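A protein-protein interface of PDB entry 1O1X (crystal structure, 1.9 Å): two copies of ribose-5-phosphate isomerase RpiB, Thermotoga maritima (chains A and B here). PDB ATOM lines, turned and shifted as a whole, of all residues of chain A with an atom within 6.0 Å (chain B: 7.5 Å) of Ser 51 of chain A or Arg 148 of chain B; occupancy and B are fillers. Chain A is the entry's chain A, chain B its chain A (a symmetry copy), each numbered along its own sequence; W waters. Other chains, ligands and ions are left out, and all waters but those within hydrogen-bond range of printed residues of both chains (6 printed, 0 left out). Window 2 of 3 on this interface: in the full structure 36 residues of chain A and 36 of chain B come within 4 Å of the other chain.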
ATOM      1  N   HIS A  21      10.129 -33.775  -1.543  1.00  0.00           N
ATOM      2  CA  HIS A  21      10.953 -34.680  -0.770  1.00  0.00           C
ATOM      3  C   HIS A  21      10.188 -35.498   0.284  1.00  0.00           C
ATOM      4  O   HIS A  21      10.583 -36.627   0.573  1.00  0.00           O
ATOM      5  CB  HIS A  21      12.075 -33.884  -0.086  1.00  0.00           C
ATOM      6  CG  HIS A  21      11.574 -32.771   0.788  1.00  0.00           C
ATOM      7  ND1 HIS A  21      10.902 -31.670   0.293  1.00  0.00           N
ATOM      8  CD2 HIS A  21      11.624 -32.609   2.133  1.00  0.00           C
ATOM      9  CE1 HIS A  21      10.549 -30.887   1.296  1.00  0.00           C
ATOM     10  NE2 HIS A  21      11.000 -31.421   2.420  1.00  0.00           N
ATOM     11  N   SER A  48      15.450 -37.117  -5.049  1.00  0.00           N
ATOM     12  CA  SER A  48      15.991 -37.437  -3.733  1.00  0.00           C
ATOM     13  C   SER A  48      15.103 -36.897  -2.598  1.00  0.00           C
ATOM     14  O   SER A  48      14.071 -36.260  -2.820  1.00  0.00           O
ATOM     15  CB  SER A  48      17.369 -36.799  -3.575  1.00  0.00           C
ATOM     16  OG  SER A  48      17.224 -35.397  -3.388  1.00  0.00           O
ATOM     17  N   GLU A  49      15.561 -37.114  -1.374  1.00  0.00           N
ATOM     18  CA  GLU A  49      14.921 -36.566  -0.200  1.00  0.00           C
ATOM     19  C   GLU A  49      15.470 -35.186   0.253  1.00  0.00           C
ATOM     20  O   GLU A  49      15.011 -34.661   1.279  1.00  0.00           O
ATOM     21  CB  GLU A  49      14.960 -37.595   0.933  1.00  0.00           C
ATOM     22  CG  GLU A  49      14.040 -38.771   0.609  1.00  0.00           C
ATOM     23  CD  GLU A  49      13.873 -39.739   1.757  1.00  0.00           C
ATOM     24  OE1 GLU A  49      14.834 -39.907   2.550  1.00  0.00           O
ATOM     25  OE2 GLU A  49      12.782 -40.348   1.841  1.00  0.00           O
ATOM     26  N   GLU A  50      16.354 -34.575  -0.536  1.00  0.00           N
ATOM     27  CA  GLU A  50      16.782 -33.209  -0.245  1.00  0.00           C
ATOM     28  C   GLU A  50      15.574 -32.277  -0.387  1.00  0.00           C
ATOM     29  O   GLU A  50      14.717 -32.449  -1.271  1.00  0.00           O
ATOM     30  CB  GLU A  50      17.922 -32.746  -1.169  1.00  0.00           C
ATOM     31  CG  GLU A  50      18.198 -31.239  -1.120  1.00  0.00           C
ATOM     32  CD  GLU A  50      19.494 -30.814  -1.800  1.00  0.00           C
ATOM     33  OE1 GLU A  50      20.455 -31.618  -1.835  1.00  0.00           O
ATOM     34  OE2 GLU A  50      19.562 -29.654  -2.284  1.00  0.00           O
ATOM     35  N   SER A  51      15.510 -31.291   0.491  1.00  0.00           N
ATOM     36  CA  SER A  51      14.345 -30.432   0.600  1.00  0.00           C
ATOM     37  C   SER A  51      14.073 -29.648  -0.687  1.00  0.00           C
ATOM     38  O   SER A  51      14.963 -29.039  -1.224  1.00  0.00           O
ATOM     39  CB  SER A  51      14.530 -29.486   1.797  1.00  0.00           C
ATOM     40  OG  SER A  51      13.447 -28.577   1.826  1.00  0.00           O
ATOM     41  N   VAL A  52      12.837 -29.702  -1.193  1.00  0.00           N
ATOM     42  CA  VAL A  52      12.408 -28.920  -2.361  1.00  0.00           C
ATOM     43  C   VAL A  52      11.015 -28.344  -2.084  1.00  0.00           C
ATOM     44  O   VAL A  52      10.391 -28.645  -1.047  1.00  0.00           O
ATOM     45  CB  VAL A  52      12.378 -29.759  -3.691  1.00  0.00           C
ATOM     46  CG1 VAL A  52      13.786 -30.282  -4.060  1.00  0.00           C
ATOM     47  CG2 VAL A  52      11.357 -30.909  -3.597  1.00  0.00           C
ATOM     48  N   ASP A  53      10.537 -27.523  -3.014  1.00  0.00           N
ATOM     49  CA  ASP A  53       9.243 -26.854  -2.863  1.00  0.00           C
ATOM     50  C   ASP A  53       8.160 -27.468  -3.789  1.00  0.00           C
ATOM     51  O   ASP A  53       8.260 -27.411  -5.022  1.00  0.00           O
ATOM     52  CB  ASP A  53       9.382 -25.356  -3.128  1.00  0.00           C
ATOM     53  CG  ASP A  53      10.403 -24.686  -2.225  1.00  0.00           C
ATOM     54  OD1 ASP A  53      10.552 -25.104  -1.047  1.00  0.00           O
ATOM     55  OD2 ASP A  53      11.091 -23.711  -2.623  1.00  0.00           O
ATOM     56  N   TYR A  54       7.098 -27.980  -3.184  1.00  0.00           N
ATOM     57  CA  TYR A  54       6.047 -28.688  -3.928  1.00  0.00           C
ATOM     58  C   TYR A  54       5.480 -27.943  -5.176  1.00  0.00           C
ATOM     59  O   TYR A  54       5.191 -28.620  -6.172  1.00  0.00           O
ATOM     60  CB  TYR A  54       4.890 -29.190  -2.990  1.00  0.00           C
ATOM     61  CG  TYR A  54       4.169 -28.130  -2.185  1.00  0.00           C
ATOM     62  CD1 TYR A  54       3.102 -27.396  -2.720  1.00  0.00           C
ATOM     63  CD2 TYR A  54       4.535 -27.868  -0.877  1.00  0.00           C
ATOM     64  CE1 TYR A  54       2.470 -26.381  -1.968  1.00  0.00           C
ATOM     65  CE2 TYR A  54       3.902 -26.865  -0.109  1.00  0.00           C
ATOM     66  CZ  TYR A  54       2.858 -26.131  -0.658  1.00  0.00           C
ATOM     67  OH  TYR A  54       2.246 -25.156   0.122  1.00  0.00           O
ATOM     68  N   PRO A  55       5.241 -26.624  -5.148  1.00  0.00           N
ATOM     69  CA  PRO A  55       4.651 -25.987  -6.347  1.00  0.00           C
ATOM     70  C   PRO A  55       5.510 -26.134  -7.622  1.00  0.00           C
ATOM     71  O   PRO A  55       4.949 -26.181  -8.711  1.00  0.00           O
ATOM     72  CB  PRO A  55       4.486 -24.499  -5.936  1.00  0.00           C
ATOM     73  CG  PRO A  55       4.455 -24.546  -4.413  1.00  0.00           C
ATOM     74  CD  PRO A  55       5.464 -25.631  -4.065  1.00  0.00           C
ATOM     75  N   ARG B  94      -6.050 -20.537  -0.395  1.00  0.00           N
ATOM     76  CA  ARG B  94      -5.451 -21.831  -0.055  1.00  0.00           C
ATOM     77  C   ARG B  94      -6.534 -22.635   0.673  1.00  0.00           C
ATOM     78  O   ARG B  94      -6.748 -22.503   1.866  1.00  0.00           O
ATOM     79  CB  ARG B  94      -4.183 -21.601   0.744  1.00  0.00           C
ATOM     80  CG  ARG B  94      -3.052 -20.946  -0.078  1.00  0.00           C
ATOM     81  CD  ARG B  94      -1.763 -20.678   0.698  1.00  0.00           C
ATOM     82  NE  ARG B  94      -2.064 -19.789   1.796  1.00  0.00           N
ATOM     83  CZ  ARG B  94      -2.227 -18.476   1.713  1.00  0.00           C
ATOM     84  NH1 ARG B  94      -2.036 -17.823   0.592  1.00  0.00           N
ATOM     85  NH2 ARG B  94      -2.630 -17.818   2.786  1.00  0.00           N
ATOM     86  N   HIS B 110       1.438 -25.340   7.988  1.00  0.00           N
ATOM     87  CA  HIS B 110       2.301 -25.399   6.814  1.00  0.00           C
ATOM     88  C   HIS B 110       1.792 -24.661   5.591  1.00  0.00           C
ATOM     89  O   HIS B 110       2.584 -24.083   4.850  1.00  0.00           O
ATOM     90  CB  HIS B 110       2.588 -26.870   6.473  1.00  0.00           C
ATOM     91  CG  HIS B 110       3.340 -27.598   7.536  1.00  0.00           C
ATOM     92  ND1 HIS B 110       3.834 -28.871   7.355  1.00  0.00           N
ATOM     93  CD2 HIS B 110       3.743 -27.209   8.773  1.00  0.00           C
ATOM     94  CE1 HIS B 110       4.488 -29.243   8.443  1.00  0.00           C
ATOM     95  NE2 HIS B 110       4.441 -28.254   9.320  1.00  0.00           N
ATOM     96  N   ASN B 111       0.486 -24.680   5.344  1.00  0.00           N
ATOM     97  CA  ASN B 111      -0.049 -24.097   4.116  1.00  0.00           C
ATOM     98  C   ASN B 111      -0.734 -22.739   4.321  1.00  0.00           C
ATOM     99  O   ASN B 111      -1.235 -22.166   3.355  1.00  0.00           O
ATOM    100  CB  ASN B 111      -1.005 -25.070   3.408  1.00  0.00           C
ATOM    101  CG  ASN B 111      -0.410 -26.458   3.209  1.00  0.00           C
ATOM    102  OD1 ASN B 111       0.406 -26.702   2.292  1.00  0.00           O
ATOM    103  ND2 ASN B 111      -0.814 -27.369   4.042  1.00  0.00           N
ATOM    104  N   GLY B 142       5.015 -20.076   9.437  1.00  0.00           N
ATOM    105  CA  GLY B 142       5.965 -19.266   8.680  1.00  0.00           C
ATOM    106  C   GLY B 142       7.162 -20.098   8.250  1.00  0.00           C
ATOM    107  O   GLY B 142       7.025 -21.139   7.630  1.00  0.00           O
ATOM    108  N   GLY B 143       8.364 -19.641   8.580  1.00  0.00           N
ATOM    109  CA  GLY B 143       9.549 -20.393   8.261  1.00  0.00           C
ATOM    110  C   GLY B 143       9.704 -20.678   6.786  1.00  0.00           C
ATOM    111  O   GLY B 143       9.426 -19.831   5.927  1.00  0.00           O
ATOM    112  N   ARG B 144      10.149 -21.897   6.482  1.00  0.00           N
ATOM    113  CA  ARG B 144      10.386 -22.340   5.134  1.00  0.00           C
ATOM    114  C   ARG B 144       9.132 -22.608   4.344  1.00  0.00           C
ATOM    115  O   ARG B 144       9.196 -22.810   3.133  1.00  0.00           O
ATOM    116  CB  ARG B 144      11.323 -23.553   5.135  1.00  0.00           C
ATOM    117  CG  ARG B 144      12.690 -23.212   5.721  1.00  0.00           C
ATOM    118  CD  ARG B 144      13.426 -22.105   4.904  1.00  0.00           C
ATOM    119  NE  ARG B 144      14.873 -22.069   5.130  1.00  0.00           N
ATOM    120  CZ  ARG B 144      15.714 -21.402   4.374  1.00  0.00           C
ATOM    121  NH1 ARG B 144      15.261 -20.684   3.347  1.00  0.00           N
ATOM    122  NH2 ARG B 144      16.977 -21.441   4.645  1.00  0.00           N
ATOM    123  N   HIS B 145       7.983 -22.578   5.013  1.00  0.00           N
ATOM    124  CA  HIS B 145       6.692 -22.788   4.333  1.00  0.00           C
ATOM    125  C   HIS B 145       6.332 -21.563   3.528  1.00  0.00           C
ATOM    126  O   HIS B 145       5.628 -21.697   2.548  1.00  0.00           O
ATOM    127  CB  HIS B 145       5.579 -23.097   5.332  1.00  0.00           C
ATOM    128  CG  HIS B 145       5.914 -24.223   6.243  1.00  0.00           C
ATOM    129  ND1 HIS B 145       6.019 -25.527   5.802  1.00  0.00           N
ATOM    130  CD2 HIS B 145       6.241 -24.235   7.559  1.00  0.00           C
ATOM    131  CE1 HIS B 145       6.385 -26.290   6.821  1.00  0.00           C
ATOM    132  NE2 HIS B 145       6.513 -25.537   7.900  1.00  0.00           N
ATOM    133  N   GLU B 146       6.803 -20.375   3.938  1.00  0.00           N
ATOM    134  CA  GLU B 146       6.369 -19.113   3.310  1.00  0.00           C
ATOM    135  C   GLU B 146       6.739 -19.066   1.819  1.00  0.00           C
ATOM    136  O   GLU B 146       5.890 -18.697   0.988  1.00  0.00           O
ATOM    137  CB  GLU B 146       6.934 -17.887   4.045  1.00  0.00           C
ATOM    138  CG  GLU B 146       6.604 -16.516   3.436  1.00  0.00           C
ATOM    139  CD  GLU B 146       5.106 -16.202   3.382  1.00  0.00           C
ATOM    140  OE1 GLU B 146       4.334 -16.804   4.151  1.00  0.00           O
ATOM    141  OE2 GLU B 146       4.691 -15.376   2.537  1.00  0.00           O
ATOM    142  N   ARG B 147       7.965 -19.477   1.489  1.00  0.00           N
ATOM    143  CA  ARG B 147       8.403 -19.554   0.095  1.00  0.00           C
ATOM    144  C   ARG B 147       7.455 -20.411  -0.762  1.00  0.00           C
ATOM    145  O   ARG B 147       7.155 -20.078  -1.912  1.00  0.00           O
ATOM    146  CB  ARG B 147       9.812 -20.099  -0.003  1.00  0.00           C
ATOM    147  CG  ARG B 147      10.340 -20.165  -1.434  1.00  0.00           C
ATOM    148  CD  ARG B 147      11.759 -20.654  -1.508  1.00  0.00           C
ATOM    149  NE  ARG B 147      12.628 -19.665  -0.895  1.00  0.00           N
ATOM    150  CZ  ARG B 147      13.894 -19.882  -0.563  1.00  0.00           C
ATOM    151  NH1 ARG B 147      14.479 -21.041  -0.825  1.00  0.00           N
ATOM    152  NH2 ARG B 147      14.578 -18.935   0.047  1.00  0.00           N
ATOM    153  N   ARG B 148       7.021 -21.522  -0.194  1.00  0.00           N
ATOM    154  CA  ARG B 148       6.169 -22.473  -0.918  1.00  0.00           C
ATOM    155  C   ARG B 148       4.811 -21.887  -1.187  1.00  0.00           C
ATOM    156  O   ARG B 148       4.325 -21.992  -2.300  1.00  0.00           O
ATOM    157  CB  ARG B 148       6.030 -23.782  -0.153  1.00  0.00           C
ATOM    158  CG  ARG B 148       7.352 -24.480  -0.096  1.00  0.00           C
ATOM    159  CD  ARG B 148       7.440 -25.501   0.970  1.00  0.00           C
ATOM    160  NE  ARG B 148       8.800 -26.038   1.067  1.00  0.00           N
ATOM    161  CZ  ARG B 148       9.261 -26.629   2.134  1.00  0.00           C
ATOM    162  NH1 ARG B 148       8.482 -26.772   3.197  1.00  0.00           N
ATOM    163  NH2 ARG B 148      10.506 -27.068   2.152  1.00  0.00           N
ATOM    164  N   ILE B 149       4.234 -21.228  -0.191  1.00  0.00           N
ATOM    165  CA  ILE B 149       2.935 -20.586  -0.370  1.00  0.00           C
ATOM    166  C   ILE B 149       2.971 -19.442  -1.390  1.00  0.00           C
ATOM    167  O   ILE B 149       2.005 -19.244  -2.184  1.00  0.00           O
ATOM    168  CB  ILE B 149       2.156 -20.285   0.940  1.00  0.00           C
ATOM    169  CG1 ILE B 149       2.757 -19.199   1.773  1.00  0.00           C
ATOM    170  CG2 ILE B 149       1.918 -21.571   1.772  1.00  0.00           C
ATOM    171  CD1 ILE B 149       1.829 -18.835   2.900  1.00  0.00           C
ATOM    172  N   ARG B 150       4.059 -18.682  -1.395  1.00  0.00           N
ATOM    173  CA  ARG B 150       4.259 -17.662  -2.437  1.00  0.00           C
ATOM    174  C   ARG B 150       4.409 -18.266  -3.855  1.00  0.00           C
ATOM    175  O   ARG B 150       3.795 -17.785  -4.827  1.00  0.00           O
ATOM    176  CB  ARG B 150       5.489 -16.822  -2.093  1.00  0.00           C
ATOM    177  CG  ARG B 150       5.297 -15.966  -0.862  1.00  0.00           C
ATOM    178  CD  ARG B 150       6.510 -15.112  -0.645  1.00  0.00           C
ATOM    179  NE  ARG B 150       6.444 -14.329   0.578  1.00  0.00           N
ATOM    180  CZ  ARG B 150       7.172 -13.248   0.816  1.00  0.00           C
ATOM    181  NH1 ARG B 150       8.043 -12.788  -0.072  1.00  0.00           N
ATOM    182  NH2 ARG B 150       7.001 -12.616   1.957  1.00  0.00           N
ATOM    183  N   LYS B 151       5.159 -19.364  -3.949  1.00  0.00           N
ATOM    184  CA  LYS B 151       5.331 -20.088  -5.214  1.00  0.00           C
ATOM    185  C   LYS B 151       4.000 -20.598  -5.797  1.00  0.00           C
ATOM    186  O   LYS B 151       3.845 -20.642  -7.024  1.00  0.00           O
ATOM    187  CB  LYS B 151       6.349 -21.234  -5.076  1.00  0.00           C
ATOM    188  CG  LYS B 151       7.793 -20.797  -5.114  1.00  0.00           C
ATOM    189  CD  LYS B 151       8.771 -21.973  -5.041  1.00  0.00           C
ATOM    190  CE  LYS B 151      10.200 -21.542  -5.231  1.00  0.00           C
ATOM    191  NZ  LYS B 151      11.113 -22.723  -5.210  1.00  0.00           N
ATOM    192  N   ILE B 152       3.045 -20.945  -4.946  1.00  0.00           N
ATOM    193  CA  ILE B 152       1.716 -21.381  -5.441  1.00  0.00           C
ATOM    194  C   ILE B 152       1.125 -20.304  -6.378  1.00  0.00           C
ATOM    195  O   ILE B 152       0.502 -20.615  -7.399  1.00  0.00           O
ATOM    196  CB  ILE B 152       0.750 -21.636  -4.267  1.00  0.00           C
ATOM    197  CG1 ILE B 152       1.190 -22.865  -3.475  1.00  0.00           C
ATOM    198  CG2 ILE B 152      -0.681 -21.795  -4.764  1.00  0.00           C
ATOM    199  CD1 ILE B 152       0.480 -22.992  -2.182  1.00  0.00           C
ATOM    200  N   ASP B 153       1.339 -19.035  -6.011  1.00  0.00           N
ATOM    201  CA  ASP B 153       0.747 -17.891  -6.707  1.00  0.00           C
ATOM    202  C   ASP B 153       1.628 -17.301  -7.767  1.00  0.00           C
ATOM    203  O   ASP B 153       1.245 -16.295  -8.380  1.00  0.00           O
ATOM    204  CB  ASP B 153       0.336 -16.803  -5.704  1.00  0.00           C
ATOM    205  CG  ASP B 153      -0.894 -17.197  -4.912  1.00  0.00           C
ATOM    206  OD1 ASP B 153      -1.713 -17.913  -5.486  1.00  0.00           O
ATOM    207  OD2 ASP B 153      -1.135 -16.807  -3.755  1.00  0.00           O
ATOM    208  N   GLU B 154       2.811 -17.884  -7.970  1.00  0.00           N
ATOM    209  CA  GLU B 154       3.667 -17.553  -9.112  1.00  0.00           C
ATOM    210  C   GLU B 154       3.264 -18.494 -10.248  1.00  0.00           C
ATOM    211  O   GLU B 154       3.899 -19.482 -10.492  1.00  0.00           O
ATOM    212  CB  GLU B 154       5.143 -17.711  -8.730  1.00  0.00           C
ATOM    213  CG  GLU B 154       5.560 -16.747  -7.630  1.00  0.00           C
ATOM    214  CD  GLU B 154       7.002 -16.936  -7.142  1.00  0.00           C
ATOM    215  OE1 GLU B 154       7.751 -17.810  -7.688  1.00  0.00           O
ATOM    216  OE2 GLU B 154       7.375 -16.212  -6.177  1.00  0.00           O
HETATM  217  O   HOH W   1      13.122 -27.010   4.433  1.00  0.00           O
HETATM  218  O   HOH W   2       3.566 -24.717   2.454  1.00  0.00           O
HETATM  219  O   HOH W   3      11.230 -23.221   1.222  1.00  0.00           O
HETATM  220  O   HOH W   4      12.809 -26.575   0.155  1.00  0.00           O
HETATM  221  O   HOH W   5       7.770 -28.970  -0.480  1.00  0.00           O
HETATM  222  O   HOH W   6      13.621 -23.412  -2.318  1.00  0.00           O
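The side-chain carboxylate of Asp 53 of chain A is in salt-bridge range of the side-chain amino group of Lys 151 of chain B, at 2.8 Å.
OD1 of Asp 53 of chain A lies within salt-bridge range of NE of Arg 148 of chain B, 2.9 Å away.
NH2 of Arg 148 of chain B is in hydrogen-bond range of OG of Ser 51 of chain A (3.3 Å).
The side-chain hydroxyl of Tyr 54 of chain A sits at hydrogen-bond distance from the side-chain amide oxygen of Asn 111 of chain B, 3.2 Å away.
The backbone carbonyl oxygen (O) of Asn 111 of chain B is in hydrogen-bond range of the guanidinium group (NE) of Arg 94 of chain B (3.0 Å).
The backbone NH (N) of Val 52 of chain A sits at hydrogen-bond distance from a ring nitrogen (ND1) of His 21 of chain A (3.1 Å).
Among the printed residues, merely in contact across the chains: Pro 55 of chain A with Arg 148 of chain B (3.3 Å), Asp 53 of chain A with Arg 147 of chain B (3.3 Å), Val 52 of chain A with Arg 148 of chain B (3.6 Å), Tyr 54 of chain A with Ile 152 of chain B (3.6 Å), Tyr 54 of chain A with Arg 148 of chain B (3.7 Å), Pro 55 of chain A with Ile 152 of chain B (3.8 Å), Pro 55 of chain A with Lys 151 of chain B (3.9 Å), His 21 of chain A with Arg 148 of chain B (3.9 Å) and Tyr 54 of chain A with Ile 149 of chain B (3.96 Å).
Glu 50 of chain A touches none of the printed residues of chain B.
Printed residues of chain B within 4 Å of Val 52 of chain A: Arg 148.
Printed residues of chain B within 4 Å of Tyr 54 of chain A: Asn 111, Arg 148, Ile 149 and Ile 152.
Arg 148 of chain B touches just these residues of chain A: His 21, Ser 51, Val 52, Asp 53, Tyr 54 and Pro 55.
The nearest residue of chain B that does not touch Ser 51 of chain A is Arg 144 of chain B (6.4 Å).
The nearest printed residue of chain A that does not touch Arg 148 of chain B is Glu 50 of chain A (7.6 Å).
Printed residues of chain A that touch a printed residue of chain B: His 21, Ser 51, Val 52, Asp 53, Tyr 54 and Pro 55.
Along chain A the printed residues that touch a printed residue of chain B span positions 21 to 55.
Of the 16 printed residues of chain B, 6 touch a printed residue of chain A.
Along chain B the printed residues that touch a printed residue of chain A span positions 111 to 152.
No position is printed for both chains.
Of the 13 pairs that touch across the chains among the printed residues, none has its exchanged pair printed and touching as well.
Water W6 bridges OD2 of Asp 53 of chain A (2.6 Å) and NH1 of Arg 147 of chain B (2.9 Å).
Water W2 bridges O of His 110 of chain B and OH of Tyr 54 of chain A.
Water W4 lies within hydrogen-bond range of the side-chain hydroxyl (OG) of Ser 51 of chain A (2.7 Å), the side-chain carboxylate (OD1) of Asp 53 of chain A (3.0 Å), the guanidinium group (NH2) of Arg 148 of chain B (3.1 Å) and the backbone carbonyl oxygen (O) of Val 52 of chain A (3.4 Å).
Water W5 lies within hydrogen-bond range of the backbone carbonyl oxygen (O) of Val 52 of chain A (2.7 Å), the backbone NH (N) of Tyr 54 of chain A (3.0 Å) and the guanidinium group (NE) of Arg 148 of chain B (3.5 Å).
Water W3 bridges O of Arg 144 of chain B (2.8 Å) and OD1 of Asp 53 of chain A (3.0 Å).
Water W1 bridges OG of Ser 51 of chain A (3.1 Å) and NH2 of Arg 148 of chain B (3.5 Å).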
